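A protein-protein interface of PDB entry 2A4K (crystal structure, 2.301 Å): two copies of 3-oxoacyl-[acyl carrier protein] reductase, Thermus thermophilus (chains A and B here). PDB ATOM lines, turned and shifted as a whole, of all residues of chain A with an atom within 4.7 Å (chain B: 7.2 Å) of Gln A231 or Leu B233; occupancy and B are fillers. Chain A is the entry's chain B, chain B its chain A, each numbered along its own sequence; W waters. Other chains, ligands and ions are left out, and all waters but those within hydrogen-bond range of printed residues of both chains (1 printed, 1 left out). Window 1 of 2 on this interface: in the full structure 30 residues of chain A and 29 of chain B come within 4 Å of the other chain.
Hydrophobic or aromatic side chains of chain A that line the printed part of chain B: Phe A219 and Ile A228.
Among the printed residues, 8 pairs touch across the chains.
Among the printed residues, no Asp or Glu carboxylate lies within 4 Å of a Lys or Arg side-chain nitrogen of the other chain.
Water W1 lies within hydrogen-bond range of the backbone carbonyl oxygen of Ala B232 (2.8 Å) and the side-chain amide nitrogen of Gln A231 (3.4 Å).
Gln A231 touches just these residues of chain B: Ala B232 (2.8 Å), Leu B233 (3.6 Å) and Tyr B234 (3.1 Å).
Of chain A, only Gln A231 comes within 4 Å of Leu B233.
Of the printed residues of chain B, Thr A229 touches Gly B238.
Of the printed residues of chain B, Phe A219 touches Phe B219.
Printed residues of chain B within 4 Å of Ile A228: Tyr B234 (3.7 Å) and Val B235 (3.99 Å).
Gly B136 touches none of the printed residues of chain A.
Leu A233 touches none of the printed residues of chain B.
The nearest residue of chain A that does not touch Leu B233 is Phe A219 (4.1 Å).
The backbone NH (N) of Leu B178 lies within hydrogen-bond range of the backbone carbonyl oxygen (O) of Leu B233, at 2.8 Å.
N of Val B235 sits at hydrogen-bond distance from O of Leu B178, at 3.0 Å.
O of Val B176 is in hydrogen-bond range of N of Leu B233, at 2.8 Å.
N of Val A176 is in hydrogen-bond range of O of Gln A231 (2.8 Å).
OG1 of Thr A229 is in hydrogen-bond range of N of Val A174, 3.0 Å away.
The backbone carbonyl oxygen (O) of Val A174 sits at hydrogen-bond distance from the backbone NH (N) of Gly A230.
Phe B219 touches its own counterpart, Phe A219.
Gln A231 touches Ala B232, but with the chains exchanged Ala A232 does not touch Gln B231 (4.2 Å).
Gln A231 touches Leu B233, but with the chains exchanged Leu A233 does not touch Gln B231 (4.2 Å).
The side-chain amide nitrogen of Gln A231 lies within hydrogen-bond range of the backbone carbonyl oxygen of Ala B232 (2.8 Å).
The backbone NH (N) of Tyr B234 sits at hydrogen-bond distance from the side-chain amide oxygen (OE1) of Gln A231 (3.1 Å).
Phe A219 touches Phe B219.
Tyr B234 touches Ile A228.
CD1 of Ile A228 touches CG2 of Val B235, 3.99 Å away.
Thr A229 touches Gly B238.
CD1 of Ile B241 touches CA of Gly A230, at 3.7 Å.
CD of Gln A231 touches CD1 of Leu B233 (3.6 Å).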
ATOM      1  N   VAL A 174     -14.022   8.246 -15.661  1.00  0.00           N
ATOM      2  CA  VAL A 174     -14.701   8.117 -14.376  1.00  0.00           C
ATOM      3  C   VAL A 174     -15.011   6.643 -14.123  1.00  0.00           C
ATOM      4  O   VAL A 174     -15.666   5.999 -14.930  1.00  0.00           O
ATOM      5  CB  VAL A 174     -15.989   8.946 -14.298  1.00  0.00           C
ATOM      6  CG1 VAL A 174     -16.541   8.935 -12.851  1.00  0.00           C
ATOM      7  CG2 VAL A 174     -15.753  10.416 -14.801  1.00  0.00           C
ATOM      8  N   ASN A 175     -14.526   6.117 -12.999  1.00  0.00           N
ATOM      9  CA  ASN A 175     -14.668   4.699 -12.671  1.00  0.00           C
ATOM     10  C   ASN A 175     -14.964   4.526 -11.189  1.00  0.00           C
ATOM     11  O   ASN A 175     -14.732   5.456 -10.391  1.00  0.00           O
ATOM     12  CB  ASN A 175     -13.396   3.938 -13.060  1.00  0.00           C
ATOM     13  CG  ASN A 175     -13.166   3.892 -14.575  1.00  0.00           C
ATOM     14  OD1 ASN A 175     -13.902   3.225 -15.311  1.00  0.00           O
ATOM     15  ND2 ASN A 175     -12.127   4.578 -15.037  1.00  0.00           N
ATOM     16  N   VAL A 176     -15.486   3.354 -10.821  1.00  0.00           N
ATOM     17  CA  VAL A 176     -15.859   3.070  -9.421  1.00  0.00           C
ATOM     18  C   VAL A 176     -15.295   1.745  -8.934  1.00  0.00           C
ATOM     19  O   VAL A 176     -15.317   0.740  -9.638  1.00  0.00           O
ATOM     20  CB  VAL A 176     -17.419   3.201  -9.159  1.00  0.00           C
ATOM     21  CG1 VAL A 176     -18.207   2.444 -10.175  1.00  0.00           C
ATOM     22  CG2 VAL A 176     -17.829   2.779  -7.696  1.00  0.00           C
ATOM     23  N   PHE A 219      -4.015   1.468 -10.524  1.00  0.00           N
ATOM     24  CA  PHE A 219      -4.262   1.038 -11.897  1.00  0.00           C
ATOM     25  C   PHE A 219      -5.156   2.047 -12.624  1.00  0.00           C
ATOM     26  O   PHE A 219      -4.813   2.506 -13.727  1.00  0.00           O
ATOM     27  CB  PHE A 219      -4.872  -0.367 -11.918  1.00  0.00           C
ATOM     28  CG  PHE A 219      -5.363  -0.804 -13.285  1.00  0.00           C
ATOM     29  CD1 PHE A 219      -4.461  -1.050 -14.329  1.00  0.00           C
ATOM     30  CD2 PHE A 219      -6.731  -0.981 -13.524  1.00  0.00           C
ATOM     31  CE1 PHE A 219      -4.924  -1.474 -15.620  1.00  0.00           C
ATOM     32  CE2 PHE A 219      -7.205  -1.404 -14.804  1.00  0.00           C
ATOM     33  CZ  PHE A 219      -6.298  -1.637 -15.853  1.00  0.00           C
ATOM     34  N   ILE A 228     -10.251   3.126 -20.283  1.00  0.00           N
ATOM     35  CA  ILE A 228     -11.222   2.478 -19.393  1.00  0.00           C
ATOM     36  C   ILE A 228     -11.985   3.553 -18.650  1.00  0.00           C
ATOM     37  O   ILE A 228     -11.436   4.265 -17.813  1.00  0.00           O
ATOM     38  CB  ILE A 228     -10.532   1.463 -18.372  1.00  0.00           C
ATOM     39  CG1 ILE A 228      -9.796   0.320 -19.123  1.00  0.00           C
ATOM     40  CG2 ILE A 228     -11.534   0.927 -17.350  1.00  0.00           C
ATOM     41  CD1 ILE A 228      -8.995  -0.640 -18.214  1.00  0.00           C
ATOM     42  N   THR A 229     -13.267   3.670 -18.960  1.00  0.00           N
ATOM     43  CA  THR A 229     -14.120   4.633 -18.286  1.00  0.00           C
ATOM     44  C   THR A 229     -15.492   3.996 -18.164  1.00  0.00           C
ATOM     45  O   THR A 229     -15.816   3.123 -18.974  1.00  0.00           O
ATOM     46  CB  THR A 229     -14.136   5.994 -19.012  1.00  0.00           C
ATOM     47  OG1 THR A 229     -14.815   6.959 -18.196  1.00  0.00           O
ATOM     48  CG2 THR A 229     -14.799   5.894 -20.429  1.00  0.00           C
ATOM     49  N   GLY A 230     -16.252   4.414 -17.138  1.00  0.00           N
ATOM     50  CA  GLY A 230     -17.592   3.887 -16.786  1.00  0.00           C
ATOM     51  C   GLY A 230     -17.650   2.535 -16.067  1.00  0.00           C
ATOM     52  O   GLY A 230     -18.723   1.948 -15.903  1.00  0.00           O
ATOM     53  N   GLN A 231     -16.498   2.044 -15.624  1.00  0.00           N
ATOM     54  CA  GLN A 231     -16.347   0.688 -15.079  1.00  0.00           C
ATOM     55  C   GLN A 231     -16.584   0.631 -13.556  1.00  0.00           C
ATOM     56  O   GLN A 231     -16.171   1.535 -12.826  1.00  0.00           O
ATOM     57  CB  GLN A 231     -14.932   0.193 -15.432  1.00  0.00           C
ATOM     58  CG  GLN A 231     -14.500  -1.129 -14.871  1.00  0.00           C
ATOM     59  CD  GLN A 231     -15.052  -2.298 -15.674  1.00  0.00           C
ATOM     60  OE1 GLN A 231     -15.326  -2.164 -16.883  1.00  0.00           O
ATOM     61  NE2 GLN A 231     -15.244  -3.449 -15.002  1.00  0.00           N
ATOM     62  N   ALA A 232     -17.260  -0.430 -13.108  1.00  0.00           N
ATOM     63  CA  ALA A 232     -17.454  -0.736 -11.704  1.00  0.00           C
ATOM     64  C   ALA A 232     -16.582  -1.937 -11.458  1.00  0.00           C
ATOM     65  O   ALA A 232     -16.818  -2.981 -12.052  1.00  0.00           O
ATOM     66  CB  ALA A 232     -18.925  -1.066 -11.403  1.00  0.00           C
ATOM     67  N   LEU A 233     -15.550  -1.783 -10.627  1.00  0.00           N
ATOM     68  CA  LEU A 233     -14.587  -2.860 -10.383  1.00  0.00           C
ATOM     69  C   LEU A 233     -14.664  -3.282  -8.927  1.00  0.00           C
ATOM     70  O   LEU A 233     -14.326  -2.506  -8.018  1.00  0.00           O
ATOM     71  CB  LEU A 233     -13.158  -2.416 -10.733  1.00  0.00           C
ATOM     72  CG  LEU A 233     -11.992  -3.419 -10.640  1.00  0.00           C
ATOM     73  CD1 LEU A 233     -12.105  -4.607 -11.612  1.00  0.00           C
ATOM     74  CD2 LEU A 233     -10.663  -2.705 -10.856  1.00  0.00           C
ATOM     75  N   GLY B 136     -13.241 -11.453 -24.486  1.00  0.00           N
ATOM     76  CA  GLY B 136     -14.421 -11.372 -25.374  1.00  0.00           C
ATOM     77  C   GLY B 136     -14.398  -9.979 -25.971  1.00  0.00           C
ATOM     78  O   GLY B 136     -13.773  -9.113 -25.396  1.00  0.00           O
ATOM     79  N   ASN B 175     -10.967 -13.902 -14.492  1.00  0.00           N
ATOM     80  CA  ASN B 175     -11.499 -12.626 -14.899  1.00  0.00           C
ATOM     81  C   ASN B 175     -11.594 -12.595 -16.414  1.00  0.00           C
ATOM     82  O   ASN B 175     -10.968 -13.411 -17.107  1.00  0.00           O
ATOM     83  CB  ASN B 175     -10.602 -11.492 -14.367  1.00  0.00           C
ATOM     84  CG  ASN B 175     -10.646 -11.366 -12.812  1.00  0.00           C
ATOM     85  OD1 ASN B 175     -11.648 -10.910 -12.236  1.00  0.00           O
ATOM     86  ND2 ASN B 175      -9.563 -11.765 -12.150  1.00  0.00           N
ATOM     87  N   VAL B 176     -12.365 -11.655 -16.942  1.00  0.00           N
ATOM     88  CA  VAL B 176     -12.451 -11.492 -18.398  1.00  0.00           C
ATOM     89  C   VAL B 176     -12.214 -10.042 -18.865  1.00  0.00           C
ATOM     90  O   VAL B 176     -12.704  -9.096 -18.260  1.00  0.00           O
ATOM     91  CB  VAL B 176     -13.769 -12.142 -18.980  1.00  0.00           C
ATOM     92  CG1 VAL B 176     -14.970 -11.666 -18.244  1.00  0.00           C
ATOM     93  CG2 VAL B 176     -13.905 -11.907 -20.532  1.00  0.00           C
ATOM     94  N   LEU B 177     -11.427  -9.911 -19.930  1.00  0.00           N
ATOM     95  CA  LEU B 177     -11.144  -8.671 -20.605  1.00  0.00           C
ATOM     96  C   LEU B 177     -12.057  -8.535 -21.811  1.00  0.00           C
ATOM     97  O   LEU B 177     -12.110  -9.447 -22.644  1.00  0.00           O
ATOM     98  CB  LEU B 177      -9.702  -8.671 -21.126  1.00  0.00           C
ATOM     99  CG  LEU B 177      -8.511  -8.386 -20.206  1.00  0.00           C
ATOM    100  CD1 LEU B 177      -7.233  -8.345 -21.032  1.00  0.00           C
ATOM    101  CD2 LEU B 177      -8.696  -7.073 -19.458  1.00  0.00           C
ATOM    102  N   LEU B 178     -12.748  -7.394 -21.903  1.00  0.00           N
ATOM    103  CA  LEU B 178     -13.655  -7.092 -23.008  1.00  0.00           C
ATOM    104  C   LEU B 178     -13.145  -5.876 -23.821  1.00  0.00           C
ATOM    105  O   LEU B 178     -13.619  -4.747 -23.632  1.00  0.00           O
ATOM    106  CB  LEU B 178     -15.098  -6.899 -22.483  1.00  0.00           C
ATOM    107  CG  LEU B 178     -15.728  -8.075 -21.682  1.00  0.00           C
ATOM    108  CD1 LEU B 178     -17.068  -7.697 -21.103  1.00  0.00           C
ATOM    109  CD2 LEU B 178     -15.919  -9.360 -22.508  1.00  0.00           C
ATOM    110  N   PRO B 179     -12.161  -6.093 -24.727  1.00  0.00           N
ATOM    111  CA  PRO B 179     -11.726  -4.940 -25.557  1.00  0.00           C
ATOM    112  C   PRO B 179     -12.828  -4.446 -26.484  1.00  0.00           C
ATOM    113  O   PRO B 179     -13.632  -5.251 -26.951  1.00  0.00           O
ATOM    114  CB  PRO B 179     -10.563  -5.510 -26.388  1.00  0.00           C
ATOM    115  CG  PRO B 179     -10.849  -7.023 -26.443  1.00  0.00           C
ATOM    116  CD  PRO B 179     -11.406  -7.323 -25.058  1.00  0.00           C
ATOM    117  N   GLN B 215      -1.820  -4.052 -21.004  1.00  0.00           N
ATOM    118  CA  GLN B 215      -1.656  -3.500 -19.658  1.00  0.00           C
ATOM    119  C   GLN B 215      -2.811  -3.944 -18.736  1.00  0.00           C
ATOM    120  O   GLN B 215      -2.584  -4.216 -17.555  1.00  0.00           O
ATOM    121  CB  GLN B 215      -1.551  -1.971 -19.690  1.00  0.00           C
ATOM    122  CG  GLN B 215      -0.243  -1.418 -20.291  1.00  0.00           C
ATOM    123  CD  GLN B 215       0.916  -1.395 -19.278  1.00  0.00           C
ATOM    124  OE1 GLN B 215       0.734  -1.700 -18.084  1.00  0.00           O
ATOM    125  NE2 GLN B 215       2.107  -1.030 -19.752  1.00  0.00           N
ATOM    126  N   ALA B 216      -4.037  -4.035 -19.267  1.00  0.00           N
ATOM    127  CA  ALA B 216      -5.167  -4.500 -18.454  1.00  0.00           C
ATOM    128  C   ALA B 216      -4.953  -5.962 -18.035  1.00  0.00           C
ATOM    129  O   ALA B 216      -5.199  -6.323 -16.885  1.00  0.00           O
ATOM    130  CB  ALA B 216      -6.486  -4.314 -19.187  1.00  0.00           C
ATOM    131  N   ALA B 217      -4.468  -6.777 -18.968  1.00  0.00           N
ATOM    132  CA  ALA B 217      -4.153  -8.172 -18.704  1.00  0.00           C
ATOM    133  C   ALA B 217      -3.011  -8.315 -17.689  1.00  0.00           C
ATOM    134  O   ALA B 217      -3.087  -9.142 -16.794  1.00  0.00           O
ATOM    135  CB  ALA B 217      -3.809  -8.897 -20.017  1.00  0.00           C
ATOM    136  N   PHE B 219      -2.214  -6.259 -15.297  1.00  0.00           N
ATOM    137  CA  PHE B 219      -2.828  -5.955 -13.986  1.00  0.00           C
ATOM    138  C   PHE B 219      -3.538  -7.188 -13.430  1.00  0.00           C
ATOM    139  O   PHE B 219      -3.335  -7.568 -12.274  1.00  0.00           O
ATOM    140  CB  PHE B 219      -3.788  -4.768 -14.071  1.00  0.00           C
ATOM    141  CG  PHE B 219      -4.600  -4.525 -12.787  1.00  0.00           C
ATOM    142  CD1 PHE B 219      -3.986  -4.027 -11.635  1.00  0.00           C
ATOM    143  CD2 PHE B 219      -5.975  -4.763 -12.759  1.00  0.00           C
ATOM    144  CE1 PHE B 219      -4.726  -3.800 -10.467  1.00  0.00           C
ATOM    145  CE2 PHE B 219      -6.726  -4.523 -11.591  1.00  0.00           C
ATOM    146  CZ  PHE B 219      -6.101  -4.048 -10.443  1.00  0.00           C
ATOM    147  N   LEU B 220      -4.329  -7.831 -14.279  1.00  0.00           N
ATOM    148  CA  LEU B 220      -5.085  -9.031 -13.890  1.00  0.00           C
ATOM    149  C   LEU B 220      -4.231 -10.287 -13.613  1.00  0.00           C
ATOM    150  O   LEU B 220      -4.631 -11.130 -12.829  1.00  0.00           O
ATOM    151  CB  LEU B 220      -6.184  -9.316 -14.921  1.00  0.00           C
ATOM    152  CG  LEU B 220      -7.360  -8.319 -14.979  1.00  0.00           C
ATOM    153  CD1 LEU B 220      -8.332  -8.714 -16.077  1.00  0.00           C
ATOM    154  CD2 LEU B 220      -8.100  -8.234 -13.631  1.00  0.00           C
ATOM    155  N   GLN B 231     -14.620 -10.812 -12.477  1.00  0.00           N
ATOM    156  CA  GLN B 231     -14.857  -9.480 -13.047  1.00  0.00           C
ATOM    157  C   GLN B 231     -14.754  -9.396 -14.576  1.00  0.00           C
ATOM    158  O   GLN B 231     -13.887 -10.017 -15.180  1.00  0.00           O
ATOM    159  CB  GLN B 231     -13.876  -8.459 -12.415  1.00  0.00           C
ATOM    160  CG  GLN B 231     -14.029  -8.319 -10.890  1.00  0.00           C
ATOM    161  CD  GLN B 231     -15.442  -7.951 -10.510  1.00  0.00           C
ATOM    162  OE1 GLN B 231     -15.923  -6.863 -10.848  1.00  0.00           O
ATOM    163  NE2 GLN B 231     -16.129  -8.869  -9.817  1.00  0.00           N
ATOM    164  N   ALA B 232     -15.643  -8.617 -15.175  1.00  0.00           N
ATOM    165  CA  ALA B 232     -15.575  -8.278 -16.588  1.00  0.00           C
ATOM    166  C   ALA B 232     -15.044  -6.854 -16.686  1.00  0.00           C
ATOM    167  O   ALA B 232     -15.699  -5.891 -16.229  1.00  0.00           O
ATOM    168  CB  ALA B 232     -16.954  -8.421 -17.274  1.00  0.00           C
ATOM    169  N   LEU B 233     -13.841  -6.741 -17.246  1.00  0.00           N
ATOM    170  CA  LEU B 233     -13.156  -5.462 -17.390  1.00  0.00           C
ATOM    171  C   LEU B 233     -13.191  -5.022 -18.848  1.00  0.00           C
ATOM    172  O   LEU B 233     -12.527  -5.619 -19.727  1.00  0.00           O
ATOM    173  CB  LEU B 233     -11.711  -5.523 -16.843  1.00  0.00           C
ATOM    174  CG  LEU B 233     -10.866  -4.227 -16.789  1.00  0.00           C
ATOM    175  CD1 LEU B 233     -11.553  -3.102 -16.011  1.00  0.00           C
ATOM    176  CD2 LEU B 233      -9.451  -4.461 -16.224  1.00  0.00           C
ATOM    177  N   TYR B 234     -13.983  -3.971 -19.078  1.00  0.00           N
ATOM    178  CA  TYR B 234     -14.195  -3.365 -20.383  1.00  0.00           C
ATOM    179  C   TYR B 234     -13.086  -2.369 -20.749  1.00  0.00           C
ATOM    180  O   TYR B 234     -12.895  -1.391 -20.035  1.00  0.00           O
ATOM    181  CB  TYR B 234     -15.533  -2.613 -20.376  1.00  0.00           C
ATOM    182  CG  TYR B 234     -16.791  -3.478 -20.287  1.00  0.00           C
ATOM    183  CD1 TYR B 234     -17.569  -3.730 -21.418  1.00  0.00           C
ATOM    184  CD2 TYR B 234     -17.202  -4.026 -19.074  1.00  0.00           C
ATOM    185  CE1 TYR B 234     -18.736  -4.497 -21.339  1.00  0.00           C
ATOM    186  CE2 TYR B 234     -18.349  -4.807 -18.985  1.00  0.00           C
ATOM    187  CZ  TYR B 234     -19.115  -5.032 -20.115  1.00  0.00           C
ATOM    188  OH  TYR B 234     -20.250  -5.800 -20.010  1.00  0.00           O
ATOM    189  N   VAL B 235     -12.384  -2.623 -21.861  1.00  0.00           N
ATOM    190  CA  VAL B 235     -11.343  -1.735 -22.394  1.00  0.00           C
ATOM    191  C   VAL B 235     -11.873  -1.243 -23.755  1.00  0.00           C
ATOM    192  O   VAL B 235     -11.428  -1.699 -24.830  1.00  0.00           O
ATOM    193  CB  VAL B 235      -9.955  -2.443 -22.498  1.00  0.00           C
ATOM    194  CG1 VAL B 235      -8.814  -1.425 -22.815  1.00  0.00           C
ATOM    195  CG2 VAL B 235      -9.636  -3.191 -21.210  1.00  0.00           C
ATOM    196  N   ASP B 236     -12.846  -0.322 -23.678  1.00  0.00           N
ATOM    197  CA  ASP B 236     -13.691   0.054 -24.822  1.00  0.00           C
ATOM    198  C   ASP B 236     -13.986   1.570 -24.923  1.00  0.00           C
ATOM    199  O   ASP B 236     -14.837   1.986 -25.714  1.00  0.00           O
ATOM    200  CB  ASP B 236     -15.022  -0.732 -24.760  1.00  0.00           C
ATOM    201  CG  ASP B 236     -15.904  -0.323 -23.578  1.00  0.00           C
ATOM    202  OD1 ASP B 236     -15.445   0.408 -22.674  1.00  0.00           O
ATOM    203  OD2 ASP B 236     -17.085  -0.728 -23.558  1.00  0.00           O
ATOM    204  N   GLY B 238     -15.593   3.338 -22.935  1.00  0.00           N
ATOM    205  CA  GLY B 238     -16.953   3.650 -22.484  1.00  0.00           C
ATOM    206  C   GLY B 238     -18.060   3.271 -23.448  1.00  0.00           C
ATOM    207  O   GLY B 238     -19.209   3.668 -23.249  1.00  0.00           O
ATOM    208  N   ILE B 241     -21.297   1.630 -22.009  1.00  0.00           N
ATOM    209  CA  ILE B 241     -22.112   2.323 -21.001  1.00  0.00           C
ATOM    210  C   ILE B 241     -23.534   2.548 -21.545  1.00  0.00           C
ATOM    211  O   ILE B 241     -24.508   2.179 -20.892  1.00  0.00           O
ATOM    212  CB  ILE B 241     -21.499   3.667 -20.506  1.00  0.00           C
ATOM    213  CG1 ILE B 241     -20.029   3.500 -20.115  1.00  0.00           C
ATOM    214  CG2 ILE B 241     -22.332   4.243 -19.330  1.00  0.00           C
ATOM    215  CD1 ILE B 241     -19.327   4.823 -19.894  1.00  0.00           C
HETATM  216  O   HOH W   1     -18.204  -5.176 -15.334  1.00  0.00           O
